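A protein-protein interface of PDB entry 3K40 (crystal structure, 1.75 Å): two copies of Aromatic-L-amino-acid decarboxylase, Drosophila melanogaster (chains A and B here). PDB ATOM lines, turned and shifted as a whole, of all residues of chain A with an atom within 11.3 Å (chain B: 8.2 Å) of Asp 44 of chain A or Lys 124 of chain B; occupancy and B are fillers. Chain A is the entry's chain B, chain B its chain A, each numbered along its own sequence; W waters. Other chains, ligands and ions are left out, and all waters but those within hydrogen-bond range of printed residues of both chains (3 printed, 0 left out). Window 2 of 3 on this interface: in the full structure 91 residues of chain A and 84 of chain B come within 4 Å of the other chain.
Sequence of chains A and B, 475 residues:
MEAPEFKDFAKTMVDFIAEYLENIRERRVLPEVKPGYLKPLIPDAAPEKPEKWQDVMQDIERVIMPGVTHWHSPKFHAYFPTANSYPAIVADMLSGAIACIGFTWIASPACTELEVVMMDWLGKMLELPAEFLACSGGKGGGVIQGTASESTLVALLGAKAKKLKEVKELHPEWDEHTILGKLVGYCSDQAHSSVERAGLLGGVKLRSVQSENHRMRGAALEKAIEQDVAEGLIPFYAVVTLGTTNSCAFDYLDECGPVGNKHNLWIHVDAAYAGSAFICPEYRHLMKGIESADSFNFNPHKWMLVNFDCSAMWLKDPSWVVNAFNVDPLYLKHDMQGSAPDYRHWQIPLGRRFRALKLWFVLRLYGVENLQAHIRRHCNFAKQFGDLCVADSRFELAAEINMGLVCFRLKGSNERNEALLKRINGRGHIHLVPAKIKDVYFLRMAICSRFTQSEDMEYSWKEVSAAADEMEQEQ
No position is printed for both chains.
Of the 11 pairs that touch across the chains among the printed residues, none has its exchanged pair printed and touching as well.
Water W1 lies within hydrogen-bond range of the backbone carbonyl oxygen of Asp 44 of chain A (2.6 Å) and the side-chain amino group of Lys 124 of chain B (3.1 Å).
Water W2 bridges the side-chain amino group (NZ) of Lys 124 of chain B (2.6 Å) and the side-chain carboxylate (OD2) of Asp 44 of chain A (3.5 Å).
Water W3 bridges O of Trp 121 of chain B (2.8 Å) and N of Ala 46 of chain A (2.9 Å).
Hydrophobic or aromatic side chains of chain A that line the printed part of chain B: Leu 38, Ile 42 and Ala 46.
Among the printed residues, no Asp or Glu carboxylate lies within 4 Å of a Lys or Arg side-chain nitrogen of the other chain.
The guanidinium group (NH2) of Arg 284 of chain B is in hydrogen-bond range of the backbone carbonyl oxygen (O) of Met 125 of chain B (2.8 Å).
Printed residues of chain B within 4 Å of Leu 38 of chain A: Val 117 (3.96 Å).
Of the printed residues of chain B, Ile 42 of chain A touches Val 117 (3.7 Å).
Of the printed residues of chain B, Pro 43 of chain A touches Trp 121.
Of chain B, only Trp 121 (3.5 Å) and Lys 124 (2.8 Å) come within 4 Å of Asp 44 of chain A.
Of the printed residues of chain A, Val 117 of chain B touches Leu 38 (3.96 Å) and Ile 42 (3.7 Å).
Met 119 of chain B touches none of the printed residues of chain A.
No residue of chain A comes within 4 Å of Asp 120 of chain B.
Of chain A, only Pro 43, Asp 44, Ala 45 and Ala 46 come within 4 Å of Trp 121 of chain B.
No residue of chain A comes within 4 Å of Gly 123 of chain B.
Lys 124 of chain B touches just one residue of chain A: Asp 44 (2.8 Å).
No residue of chain A comes within 4 Å of Cys 135 of chain B.
The nearest residue of chain B that does not touch Asp 44 of chain A is Asp 120 of chain B (5.4 Å).
The nearest residue of chain A that does not touch Lys 124 of chain B is Ala 45 of chain A (4.6 Å).
The nearest printed residue of chain B that does not touch Ile 42 of chain A is Met 118 of chain B (4.01 Å).
The indole nitrogen (NE1) of Trp 121 of chain B sits at hydrogen-bond distance from the backbone carbonyl oxygen (O) of Pro 43 of chain A (2.9 Å).
N of Val 368 of chain B is in hydrogen-bond range of O of Glu 48 of chain A (3.3 Å).
N of Val 368 of chain B sits at hydrogen-bond distance from O of Pro 47 of chain A.
The side-chain amino group of Lys 124 of chain B sits at hydrogen-bond distance from the backbone carbonyl oxygen of Asp 44 of chain A, at 2.8 Å.
The backbone NH (N) of Ala 45 of chain A lies close to the indole nitrogen (NE1) of Trp 121 of chain B (3.4 Å).
Among the printed residues, merely in contact across the chains: Asp 44 of chain A with Trp 121 of chain B, Ala 46 of chain A with Trp 121 of chain B, Ile 42 of chain A with Val 117 of chain B, Ala 46 of chain A with Val 368 of chain B, Ala 46 of chain A with Met 125 of chain B and Leu 38 of chain A with Val 117 of chain B.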
ATOM      1  N   LEU A  38      -0.618   3.897 -34.914  1.00  0.00           N
ATOM      2  CA  LEU A  38      -1.642   4.120 -33.872  1.00  0.00           C
ATOM      3  C   LEU A  38      -1.196   5.101 -32.782  1.00  0.00           C
ATOM      4  O   LEU A  38      -1.963   5.985 -32.393  1.00  0.00           O
ATOM      5  CB  LEU A  38      -2.100   2.785 -33.262  1.00  0.00           C
ATOM      6  CG  LEU A  38      -3.307   2.816 -32.328  1.00  0.00           C
ATOM      7  CD1 LEU A  38      -4.118   1.533 -32.455  1.00  0.00           C
ATOM      8  CD2 LEU A  38      -2.779   2.919 -30.898  1.00  0.00           C
ATOM      9  N   LYS A  39       0.033   4.944 -32.299  1.00  0.00           N
ATOM     10  CA  LYS A  39       0.518   5.774 -31.188  1.00  0.00           C
ATOM     11  C   LYS A  39       0.284   7.283 -31.410  1.00  0.00           C
ATOM     12  O   LYS A  39      -0.245   7.943 -30.505  1.00  0.00           O
ATOM     13  CB  LYS A  39       1.987   5.451 -30.896  1.00  0.00           C
ATOM     14  CG  LYS A  39       2.680   6.297 -29.839  1.00  0.00           C
ATOM     15  CD  LYS A  39       4.111   5.795 -29.657  1.00  0.00           C
ATOM     16  CE  LYS A  39       4.929   6.677 -28.719  1.00  0.00           C
ATOM     17  NZ  LYS A  39       6.139   5.971 -28.219  1.00  0.00           N
ATOM     18  N   PRO A  40       0.623   7.825 -32.619  1.00  0.00           N
ATOM     19  CA  PRO A  40       0.438   9.278 -32.822  1.00  0.00           C
ATOM     20  C   PRO A  40      -1.021   9.735 -32.837  1.00  0.00           C
ATOM     21  O   PRO A  40      -1.287  10.943 -32.774  1.00  0.00           O
ATOM     22  CB  PRO A  40       1.058   9.538 -34.215  1.00  0.00           C
ATOM     23  CG  PRO A  40       1.766   8.263 -34.616  1.00  0.00           C
ATOM     24  CD  PRO A  40       1.184   7.151 -33.815  1.00  0.00           C
ATOM     25  N   LEU A  41      -1.958   8.792 -32.944  1.00  0.00           N
ATOM     26  CA  LEU A  41      -3.373   9.111 -33.063  1.00  0.00           C
ATOM     27  C   LEU A  41      -4.064   9.287 -31.725  1.00  0.00           C
ATOM     28  O   LEU A  41      -5.160   9.831 -31.659  1.00  0.00           O
ATOM     29  CB  LEU A  41      -4.098   8.024 -33.859  1.00  0.00           C
ATOM     30  CG  LEU A  41      -3.765   7.978 -35.354  1.00  0.00           C
ATOM     31  CD1 LEU A  41      -4.577   6.864 -35.993  1.00  0.00           C
ATOM     32  CD2 LEU A  41      -4.084   9.356 -35.994  1.00  0.00           C
ATOM     33  N   ILE A  42      -3.434   8.797 -30.662  1.00  0.00           N
ATOM     34  CA  ILE A  42      -4.026   8.880 -29.330  1.00  0.00           C
ATOM     35  C   ILE A  42      -3.033   9.440 -28.276  1.00  0.00           C
ATOM     36  O   ILE A  42      -1.802   9.420 -28.492  1.00  0.00           O
ATOM     37  CB  ILE A  42      -4.645   7.513 -28.865  1.00  0.00           C
ATOM     38  CG1 ILE A  42      -3.562   6.450 -28.688  1.00  0.00           C
ATOM     39  CG2 ILE A  42      -5.781   7.024 -29.825  1.00  0.00           C
ATOM     40  CD1 ILE A  42      -4.126   5.144 -28.080  1.00  0.00           C
ATOM     41  N   PRO A  43      -3.564   9.979 -27.161  1.00  0.00           N
ATOM     42  CA  PRO A  43      -2.708  10.563 -26.107  1.00  0.00           C
ATOM     43  C   PRO A  43      -1.673   9.625 -25.480  1.00  0.00           C
ATOM     44  O   PRO A  43      -1.801   8.405 -25.558  1.00  0.00           O
ATOM     45  CB  PRO A  43      -3.727  11.059 -25.057  1.00  0.00           C
ATOM     46  CG  PRO A  43      -4.991  11.244 -25.817  1.00  0.00           C
ATOM     47  CD  PRO A  43      -4.996  10.130 -26.831  1.00  0.00           C
ATOM     48  N   ASP A  44      -0.631  10.177 -24.870  1.00  0.00           N
ATOM     49  CA  ASP A  44       0.391   9.305 -24.324  1.00  0.00           C
ATOM     50  C   ASP A  44       0.106   8.836 -22.911  1.00  0.00           C
ATOM     51  O   ASP A  44       0.865   8.041 -22.389  1.00  0.00           O
ATOM     52  CB  ASP A  44       1.803   9.876 -24.453  1.00  0.00           C
ATOM     53  CG  ASP A  44       1.935  11.213 -23.829  1.00  0.00           C
ATOM     54  OD1 ASP A  44       2.855  11.965 -24.247  1.00  0.00           O
ATOM     55  OD2 ASP A  44       1.110  11.530 -22.942  1.00  0.00           O
ATOM     56  N   ALA A  45      -0.987   9.328 -22.320  1.00  0.00           N
ATOM     57  CA  ALA A  45      -1.430   8.903 -20.982  1.00  0.00           C
ATOM     58  C   ALA A  45      -2.934   8.852 -20.890  1.00  0.00           C
ATOM     59  O   ALA A  45      -3.639   9.532 -21.637  1.00  0.00           O
ATOM     60  CB  ALA A  45      -0.887   9.838 -19.896  1.00  0.00           C
ATOM     61  N   ALA A  46      -3.446   8.054 -19.947  1.00  0.00           N
ATOM     62  CA  ALA A  46      -4.858   8.023 -19.647  1.00  0.00           C
ATOM     63  C   ALA A  46      -5.408   9.431 -19.256  1.00  0.00           C
ATOM     64  O   ALA A  46      -4.645  10.239 -18.693  1.00  0.00           O
ATOM     65  CB  ALA A  46      -5.150   7.002 -18.538  1.00  0.00           C
ATOM     66  N   PRO A  47      -6.682   9.723 -19.568  1.00  0.00           N
ATOM     67  CA  PRO A  47      -7.235  11.024 -19.177  1.00  0.00           C
ATOM     68  C   PRO A  47      -7.509  11.071 -17.685  1.00  0.00           C
ATOM     69  O   PRO A  47      -7.899  10.063 -17.090  1.00  0.00           O
ATOM     70  CB  PRO A  47      -8.541  11.095 -19.951  1.00  0.00           C
ATOM     71  CG  PRO A  47      -8.996   9.618 -20.029  1.00  0.00           C
ATOM     72  CD  PRO A  47      -7.696   8.893 -20.265  1.00  0.00           C
ATOM     73  N   GLU A  48      -7.287  12.239 -17.077  1.00  0.00           N
ATOM     74  CA  GLU A  48      -7.594  12.397 -15.656  1.00  0.00           C
ATOM     75  C   GLU A  48      -9.087  12.379 -15.393  1.00  0.00           C
ATOM     76  O   GLU A  48      -9.531  11.766 -14.424  1.00  0.00           O
ATOM     77  CB  GLU A  48      -6.940  13.675 -15.124  1.00  0.00           C
ATOM     78  CG  GLU A  48      -5.449  13.540 -15.008  1.00  0.00           C
ATOM     79  CD  GLU A  48      -5.042  12.493 -13.979  1.00  0.00           C
ATOM     80  OE1 GLU A  48      -5.570  12.525 -12.836  1.00  0.00           O
ATOM     81  OE2 GLU A  48      -4.203  11.643 -14.304  1.00  0.00           O
ATOM     82  N   GLU A  51     -13.849  10.942 -20.355  1.00  0.00           N
ATOM     83  CA  GLU A  51     -14.195  11.408 -21.713  1.00  0.00           C
ATOM     84  C   GLU A  51     -15.643  11.042 -22.063  1.00  0.00           C
ATOM     85  O   GLU A  51     -16.309  10.330 -21.308  1.00  0.00           O
ATOM     86  CB  GLU A  51     -13.231  10.791 -22.725  1.00  0.00           C
ATOM     87  CG  GLU A  51     -11.793  11.160 -22.543  1.00  0.00           C
ATOM     88  CD  GLU A  51     -10.966  10.667 -23.695  1.00  0.00           C
ATOM     89  OE1 GLU A  51     -10.160   9.757 -23.487  1.00  0.00           O
ATOM     90  OE2 GLU A  51     -11.160  11.168 -24.833  1.00  0.00           O
ATOM     91  N   ARG A  62     -11.907   6.133 -36.865  1.00  0.00           N
ATOM     92  CA  ARG A  62     -10.680   6.929 -37.003  1.00  0.00           C
ATOM     93  C   ARG A  62      -9.374   6.203 -36.603  1.00  0.00           C
ATOM     94  O   ARG A  62      -8.365   6.309 -37.296  1.00  0.00           O
ATOM     95  CB  ARG A  62     -10.808   8.240 -36.218  1.00  0.00           C
ATOM     96  CG  ARG A  62      -9.600   9.181 -36.355  1.00  0.00           C
ATOM     97  CD  ARG A  62      -9.740  10.453 -35.497  1.00  0.00           C
ATOM     98  NE  ARG A  62      -9.456  10.199 -34.081  1.00  0.00           N
ATOM     99  CZ  ARG A  62      -8.239  10.219 -33.540  1.00  0.00           C
ATOM    100  NH1 ARG A  62      -7.159  10.473 -34.283  1.00  0.00           N
ATOM    101  NH2 ARG A  62      -8.102   9.968 -32.244  1.00  0.00           N
ATOM    102  N   VAL B 117       0.109   0.562 -26.296  1.00  0.00           N
ATOM    103  CA  VAL B 117      -0.187   1.886 -25.732  1.00  0.00           C
ATOM    104  C   VAL B 117      -0.977   1.727 -24.410  1.00  0.00           C
ATOM    105  O   VAL B 117      -0.677   2.405 -23.430  1.00  0.00           O
ATOM    106  CB  VAL B 117      -0.902   2.820 -26.728  1.00  0.00           C
ATOM    107  CG1 VAL B 117      -1.186   4.204 -26.108  1.00  0.00           C
ATOM    108  CG2 VAL B 117      -0.063   2.966 -28.014  1.00  0.00           C
ATOM    109  N   MET B 118      -1.968   0.835 -24.374  1.00  0.00           N
ATOM    110  CA  MET B 118      -2.774   0.694 -23.120  1.00  0.00           C
ATOM    111  C   MET B 118      -1.925   0.206 -21.950  1.00  0.00           C
ATOM    112  O   MET B 118      -2.134   0.600 -20.789  1.00  0.00           O
ATOM    113  CB  MET B 118      -3.986  -0.223 -23.347  1.00  0.00           C
ATOM    114  CG  MET B 118      -5.051   0.433 -24.272  1.00  0.00           C
ATOM    115  SD  MET B 118      -5.573   2.060 -23.622  1.00  0.00           S
ATOM    116  CE  MET B 118      -4.544   3.154 -24.626  1.00  0.00           C
ATOM    117  N   MET B 119      -0.984  -0.676 -22.240  1.00  0.00           N
ATOM    118  CA  MET B 119      -0.100  -1.144 -21.165  1.00  0.00           C
ATOM    119  C   MET B 119       0.828  -0.041 -20.703  1.00  0.00           C
ATOM    120  O   MET B 119       1.217  -0.030 -19.547  1.00  0.00           O
ATOM    121  CB  MET B 119       0.657  -2.407 -21.560  1.00  0.00           C
ATOM    122  CG  MET B 119      -0.316  -3.593 -21.629  1.00  0.00           C
ATOM    123  SD  MET B 119      -1.043  -4.068 -20.020  1.00  0.00           S
ATOM    124  CE  MET B 119       0.378  -4.847 -19.273  1.00  0.00           C
ATOM    125  N   ASP B 120       1.159   0.881 -21.605  1.00  0.00           N
ATOM    126  CA  ASP B 120       1.917   2.067 -21.184  1.00  0.00           C
ATOM    127  C   ASP B 120       1.061   3.002 -20.363  1.00  0.00           C
ATOM    128  O   ASP B 120       1.536   3.500 -19.337  1.00  0.00           O
ATOM    129  CB  ASP B 120       2.544   2.799 -22.367  1.00  0.00           C
ATOM    130  CG  ASP B 120       3.854   2.164 -22.812  1.00  0.00           C
ATOM    131  OD1 ASP B 120       4.344   1.213 -22.177  1.00  0.00           O
ATOM    132  OD2 ASP B 120       4.384   2.616 -23.842  1.00  0.00           O
ATOM    133  N   TRP B 121      -0.200   3.198 -20.761  1.00  0.00           N
ATOM    134  CA  TRP B 121      -1.126   4.067 -19.998  1.00  0.00           C
ATOM    135  C   TRP B 121      -1.249   3.514 -18.583  1.00  0.00           C
ATOM    136  O   TRP B 121      -1.120   4.235 -17.582  1.00  0.00           O
ATOM    137  CB  TRP B 121      -2.505   4.039 -20.634  1.00  0.00           C
ATOM    138  CG  TRP B 121      -2.707   4.990 -21.784  1.00  0.00           C
ATOM    139  CD1 TRP B 121      -1.754   5.587 -22.576  1.00  0.00           C
ATOM    140  CD2 TRP B 121      -3.976   5.443 -22.253  1.00  0.00           C
ATOM    141  NE1 TRP B 121      -2.374   6.442 -23.489  1.00  0.00           N
ATOM    142  CE2 TRP B 121      -3.732   6.352 -23.329  1.00  0.00           C
ATOM    143  CE3 TRP B 121      -5.306   5.180 -21.866  1.00  0.00           C
ATOM    144  CZ2 TRP B 121      -4.778   6.976 -24.046  1.00  0.00           C
ATOM    145  CZ3 TRP B 121      -6.348   5.820 -22.555  1.00  0.00           C
ATOM    146  CH2 TRP B 121      -6.075   6.719 -23.639  1.00  0.00           C
ATOM    147  N   LEU B 122      -1.482   2.208 -18.495  1.00  0.00           N
ATOM    148  CA  LEU B 122      -1.723   1.574 -17.197  1.00  0.00           C
ATOM    149  C   LEU B 122      -0.434   1.499 -16.393  1.00  0.00           C
ATOM    150  O   LEU B 122      -0.451   1.764 -15.186  1.00  0.00           O
ATOM    151  CB  LEU B 122      -2.326   0.180 -17.406  1.00  0.00           C
ATOM    152  CG  LEU B 122      -2.847  -0.513 -16.169  1.00  0.00           C
ATOM    153  CD1 LEU B 122      -3.862   0.358 -15.373  1.00  0.00           C
ATOM    154  CD2 LEU B 122      -3.514  -1.830 -16.646  1.00  0.00           C
ATOM    155  N   GLY B 123       0.697   1.237 -17.058  1.00  0.00           N
ATOM    156  CA  GLY B 123       1.993   1.217 -16.389  1.00  0.00           C
ATOM    157  C   GLY B 123       2.333   2.587 -15.807  1.00  0.00           C
ATOM    158  O   GLY B 123       2.818   2.681 -14.668  1.00  0.00           O
ATOM    159  N   LYS B 124       2.054   3.651 -16.548  1.00  0.00           N
ATOM    160  CA  LYS B 124       2.233   5.021 -15.997  1.00  0.00           C
ATOM    161  C   LYS B 124       1.318   5.281 -14.800  1.00  0.00           C
ATOM    162  O   LYS B 124       1.713   5.954 -13.821  1.00  0.00           O
ATOM    163  CB  LYS B 124       1.966   6.048 -17.083  1.00  0.00           C
ATOM    164  CG  LYS B 124       3.047   6.042 -18.159  1.00  0.00           C
ATOM    165  CD  LYS B 124       2.661   6.982 -19.301  1.00  0.00           C
ATOM    166  CE  LYS B 124       3.643   6.813 -20.426  1.00  0.00           C
ATOM    167  NZ  LYS B 124       3.513   7.930 -21.402  1.00  0.00           N
ATOM    168  N   MET B 125       0.100   4.760 -14.878  1.00  0.00           N
ATOM    169  CA  MET B 125      -0.839   4.944 -13.771  1.00  0.00           C
ATOM    170  C   MET B 125      -0.310   4.335 -12.496  1.00  0.00           C
ATOM    171  O   MET B 125      -0.564   4.846 -11.388  1.00  0.00           O
ATOM    172  CB  MET B 125      -2.204   4.351 -14.125  1.00  0.00           C
ATOM    173  CG  MET B 125      -3.003   5.272 -15.056  1.00  0.00           C
ATOM    174  SD  MET B 125      -4.446   4.449 -15.739  1.00  0.00           S
ATOM    175  CE  MET B 125      -5.300   3.984 -14.229  1.00  0.00           C
ATOM    176  N   LEU B 126       0.390   3.217 -12.633  1.00  0.00           N
ATOM    177  CA  LEU B 126       0.979   2.503 -11.491  1.00  0.00           C
ATOM    178  C   LEU B 126       2.355   3.024 -11.102  1.00  0.00           C
ATOM    179  O   LEU B 126       2.986   2.490 -10.209  1.00  0.00           O
ATOM    180  CB  LEU B 126       1.121   0.999 -11.849  1.00  0.00           C
ATOM    181  CG  LEU B 126      -0.151   0.232 -12.172  1.00  0.00           C
ATOM    182  CD1 LEU B 126       0.272  -1.084 -12.920  1.00  0.00           C
ATOM    183  CD2 LEU B 126      -0.767  -0.122 -10.902  1.00  0.00           C
ATOM    184  N   GLU B 127       2.824   4.042 -11.802  1.00  0.00           N
ATOM    185  CA  GLU B 127       4.226   4.508 -11.673  1.00  0.00           C
ATOM    186  C   GLU B 127       5.248   3.365 -11.741  1.00  0.00           C
ATOM    187  O   GLU B 127       6.191   3.267 -10.923  1.00  0.00           O
ATOM    188  CB  GLU B 127       4.402   5.329 -10.390  1.00  0.00           C
ATOM    189  CG  GLU B 127       3.772   6.658 -10.494  1.00  0.00           C
ATOM    190  CD  GLU B 127       4.260   7.634  -9.417  1.00  0.00           C
ATOM    191  OE1 GLU B 127       4.958   7.230  -8.456  1.00  0.00           O
ATOM    192  OE2 GLU B 127       3.910   8.810  -9.562  1.00  0.00           O
ATOM    193  N   LEU B 128       5.085   2.477 -12.726  1.00  0.00           N
ATOM    194  CA  LEU B 128       6.042   1.397 -12.871  1.00  0.00           C
ATOM    195  C   LEU B 128       7.361   1.972 -13.327  1.00  0.00           C
ATOM    196  O   LEU B 128       7.373   3.003 -14.020  1.00  0.00           O
ATOM    197  CB  LEU B 128       5.602   0.350 -13.900  1.00  0.00           C
ATOM    198  CG  LEU B 128       4.396  -0.525 -13.527  1.00  0.00           C
ATOM    199  CD1 LEU B 128       4.135  -1.586 -14.634  1.00  0.00           C
ATOM    200  CD2 LEU B 128       4.573  -1.219 -12.182  1.00  0.00           C
ATOM    201  N   PRO B 129       8.462   1.325 -12.939  1.00  0.00           N
ATOM    202  CA  PRO B 129       9.784   1.722 -13.458  1.00  0.00           C
ATOM    203  C   PRO B 129       9.787   1.820 -14.983  1.00  0.00           C
ATOM    204  O   PRO B 129       9.075   1.050 -15.660  1.00  0.00           O
ATOM    205  CB  PRO B 129      10.694   0.601 -12.970  1.00  0.00           C
ATOM    206  CG  PRO B 129      10.097   0.200 -11.675  1.00  0.00           C
ATOM    207  CD  PRO B 129       8.583   0.224 -11.967  1.00  0.00           C
ATOM    208  N   PHE B 132       9.832  -1.071 -17.645  1.00  0.00           N
ATOM    209  CA  PHE B 132       8.627  -1.841 -18.007  1.00  0.00           C
ATOM    210  C   PHE B 132       7.785  -1.168 -19.083  1.00  0.00           C
ATOM    211  O   PHE B 132       6.833  -1.776 -19.588  1.00  0.00           O
ATOM    212  CB  PHE B 132       7.726  -2.093 -16.771  1.00  0.00           C
ATOM    213  CG  PHE B 132       8.312  -3.013 -15.730  1.00  0.00           C
ATOM    214  CD1 PHE B 132       8.404  -4.379 -15.940  1.00  0.00           C
ATOM    215  CD2 PHE B 132       8.747  -2.487 -14.509  1.00  0.00           C
ATOM    216  CE1 PHE B 132       8.935  -5.228 -14.955  1.00  0.00           C
ATOM    217  CE2 PHE B 132       9.278  -3.315 -13.514  1.00  0.00           C
ATOM    218  CZ  PHE B 132       9.370  -4.689 -13.734  1.00  0.00           C
ATOM    219  N   LEU B 133       8.109   0.076 -19.441  1.00  0.00           N
ATOM    220  CA  LEU B 133       7.290   0.864 -20.366  1.00  0.00           C
ATOM    221  C   LEU B 133       7.835   0.758 -21.796  1.00  0.00           C
ATOM    222  O   LEU B 133       9.041   0.939 -22.009  1.00  0.00           O
ATOM    223  CB  LEU B 133       7.225   2.328 -19.894  1.00  0.00           C
ATOM    224  CG  LEU B 133       6.679   2.551 -18.464  1.00  0.00           C
ATOM    225  CD1 LEU B 133       6.520   4.041 -18.125  1.00  0.00           C
ATOM    226  CD2 LEU B 133       5.350   1.830 -18.309  1.00  0.00           C
ATOM    227  N   ALA B 134       6.976   0.421 -22.760  1.00  0.00           N
ATOM    228  CA  ALA B 134       7.433   0.309 -24.153  1.00  0.00           C
ATOM    229  C   ALA B 134       7.902   1.659 -24.667  1.00  0.00           C
ATOM    230  O   ALA B 134       8.851   1.724 -25.458  1.00  0.00           O
ATOM    231  CB  ALA B 134       6.330  -0.247 -25.069  1.00  0.00           C
ATOM    232  N   CYS B 135       7.251   2.726 -24.207  1.00  0.00           N
ATOM    233  CA  CYS B 135       7.524   4.081 -24.683  1.00  0.00           C
ATOM    234  C   CYS B 135       8.887   4.604 -24.218  1.00  0.00           C
ATOM    235  O   CYS B 135       9.345   5.643 -24.702  1.00  0.00           O
ATOM    236  CB  CYS B 135       6.400   5.051 -24.292  1.00  0.00           C
ATOM    237  SG  CYS B 135       6.104   5.166 -22.490  1.00  0.00           S
ATOM    238  N   SER B 136       9.529   3.889 -23.297  1.00  0.00           N
ATOM    239  CA  SER B 136      10.892   4.233 -22.895  1.00  0.00           C
ATOM    240  C   SER B 136      11.929   3.804 -23.957  1.00  0.00           C
ATOM    241  O   SER B 136      13.070   4.251 -23.923  1.00  0.00           O
ATOM    242  CB  SER B 136      11.208   3.641 -21.522  1.00  0.00           C
ATOM    243  OG  SER B 136      11.594   2.286 -21.628  1.00  0.00           O
ATOM    244  N   PHE B 278      -2.526   0.272  -6.582  1.00  0.00           N
ATOM    245  CA  PHE B 278      -1.264   0.994  -6.846  1.00  0.00           C
ATOM    246  C   PHE B 278      -1.394   2.186  -7.793  1.00  0.00           C
ATOM    247  O   PHE B 278      -0.410   2.920  -7.999  1.00  0.00           O
ATOM    248  CB  PHE B 278      -0.158   0.009  -7.311  1.00  0.00           C
ATOM    249  CG  PHE B 278       0.096  -1.138  -6.377  1.00  0.00           C
ATOM    250  CD1 PHE B 278      -0.288  -1.112  -5.015  1.00  0.00           C
ATOM    251  CD2 PHE B 278       0.734  -2.283  -6.868  1.00  0.00           C
ATOM    252  CE1 PHE B 278      -0.064  -2.235  -4.191  1.00  0.00           C
ATOM    253  CE2 PHE B 278       1.006  -3.377  -6.025  1.00  0.00           C
ATOM    254  CZ  PHE B 278       0.615  -3.361  -4.727  1.00  0.00           C
ATOM    255  N   ILE B 279      -2.594   2.408  -8.332  1.00  0.00           N
ATOM    256  CA  ILE B 279      -2.879   3.631  -9.091  1.00  0.00           C
ATOM    257  C   ILE B 279      -3.038   4.835  -8.112  1.00  0.00           C
ATOM    258  O   ILE B 279      -3.074   5.968  -8.556  1.00  0.00           O
ATOM    259  CB  ILE B 279      -4.140   3.504  -9.977  1.00  0.00           C
ATOM    260  CG1 ILE B 279      -5.422   3.407  -9.155  1.00  0.00           C
ATOM    261  CG2 ILE B 279      -3.944   2.319 -11.002  1.00  0.00           C
ATOM    262  CD1 ILE B 279      -6.768   3.279 -10.001  1.00  0.00           C
ATOM    263  N   ARG B 284       1.177   2.973  -3.132  1.00  0.00           N
ATOM    264  CA  ARG B 284       2.372   2.546  -3.912  1.00  0.00           C
ATOM    265  C   ARG B 284       3.549   2.043  -3.109  1.00  0.00           C
ATOM    266  O   ARG B 284       4.335   1.240  -3.626  1.00  0.00           O
ATOM    267  CB  ARG B 284       2.802   3.627  -4.868  1.00  0.00           C
ATOM    268  CG  ARG B 284       1.799   3.878  -5.890  1.00  0.00           C
ATOM    269  CD  ARG B 284       2.384   4.684  -7.023  1.00  0.00           C
ATOM    270  NE  ARG B 284       1.318   5.036  -7.954  1.00  0.00           N
ATOM    271  CZ  ARG B 284       0.972   6.267  -8.269  1.00  0.00           C
ATOM    272  NH1 ARG B 284       1.639   7.302  -7.761  1.00  0.00           N
ATOM    273  NH2 ARG B 284      -0.006   6.461  -9.135  1.00  0.00           N
ATOM    274  N   TRP B 314       3.594  -7.072 -17.036  1.00  0.00           N
ATOM    275  CA  TRP B 314       4.724  -6.335 -17.611  1.00  0.00           C
ATOM    276  C   TRP B 314       5.969  -7.171 -17.399  1.00  0.00           C
ATOM    277  O   TRP B 314       6.066  -7.920 -16.418  1.00  0.00           O
ATOM    278  CB  TRP B 314       4.888  -4.971 -16.937  1.00  0.00           C
ATOM    279  CG  TRP B 314       3.837  -3.947 -17.271  1.00  0.00           C
ATOM    280  CD1 TRP B 314       3.930  -2.939 -18.197  1.00  0.00           C
ATOM    281  CD2 TRP B 314       2.549  -3.824 -16.669  1.00  0.00           C
ATOM    282  NE1 TRP B 314       2.798  -2.193 -18.194  1.00  0.00           N
ATOM    283  CE2 TRP B 314       1.928  -2.699 -17.256  1.00  0.00           C
ATOM    284  CE3 TRP B 314       1.864  -4.544 -15.674  1.00  0.00           C
ATOM    285  CZ2 TRP B 314       0.629  -2.307 -16.930  1.00  0.00           C
ATOM    286  CZ3 TRP B 314       0.572  -4.137 -15.323  1.00  0.00           C
ATOM    287  CH2 TRP B 314      -0.023  -3.010 -15.952  1.00  0.00           C
ATOM    288  N   VAL B 368      -8.626   8.611 -14.741  1.00  0.00           N
ATOM    289  CA  VAL B 368      -7.777   8.187 -13.624  1.00  0.00           C
ATOM    290  C   VAL B 368      -8.419   8.554 -12.283  1.00  0.00           C
ATOM    291  O   VAL B 368      -8.498   7.718 -11.366  1.00  0.00           O
ATOM    292  CB  VAL B 368      -6.363   8.759 -13.734  1.00  0.00           C
ATOM    293  CG1 VAL B 368      -5.536   8.312 -12.499  1.00  0.00           C
ATOM    294  CG2 VAL B 368      -5.689   8.318 -15.066  1.00  0.00           C
HETATM  295  O   HOH W   1       2.220   6.275 -23.647  1.00  0.00           O
HETATM  296  O   HOH W   2       3.208  10.364 -20.403  1.00  0.00           O
HETATM  297  O   HOH W   3      -1.580   6.919 -18.008  1.00  0.00           O
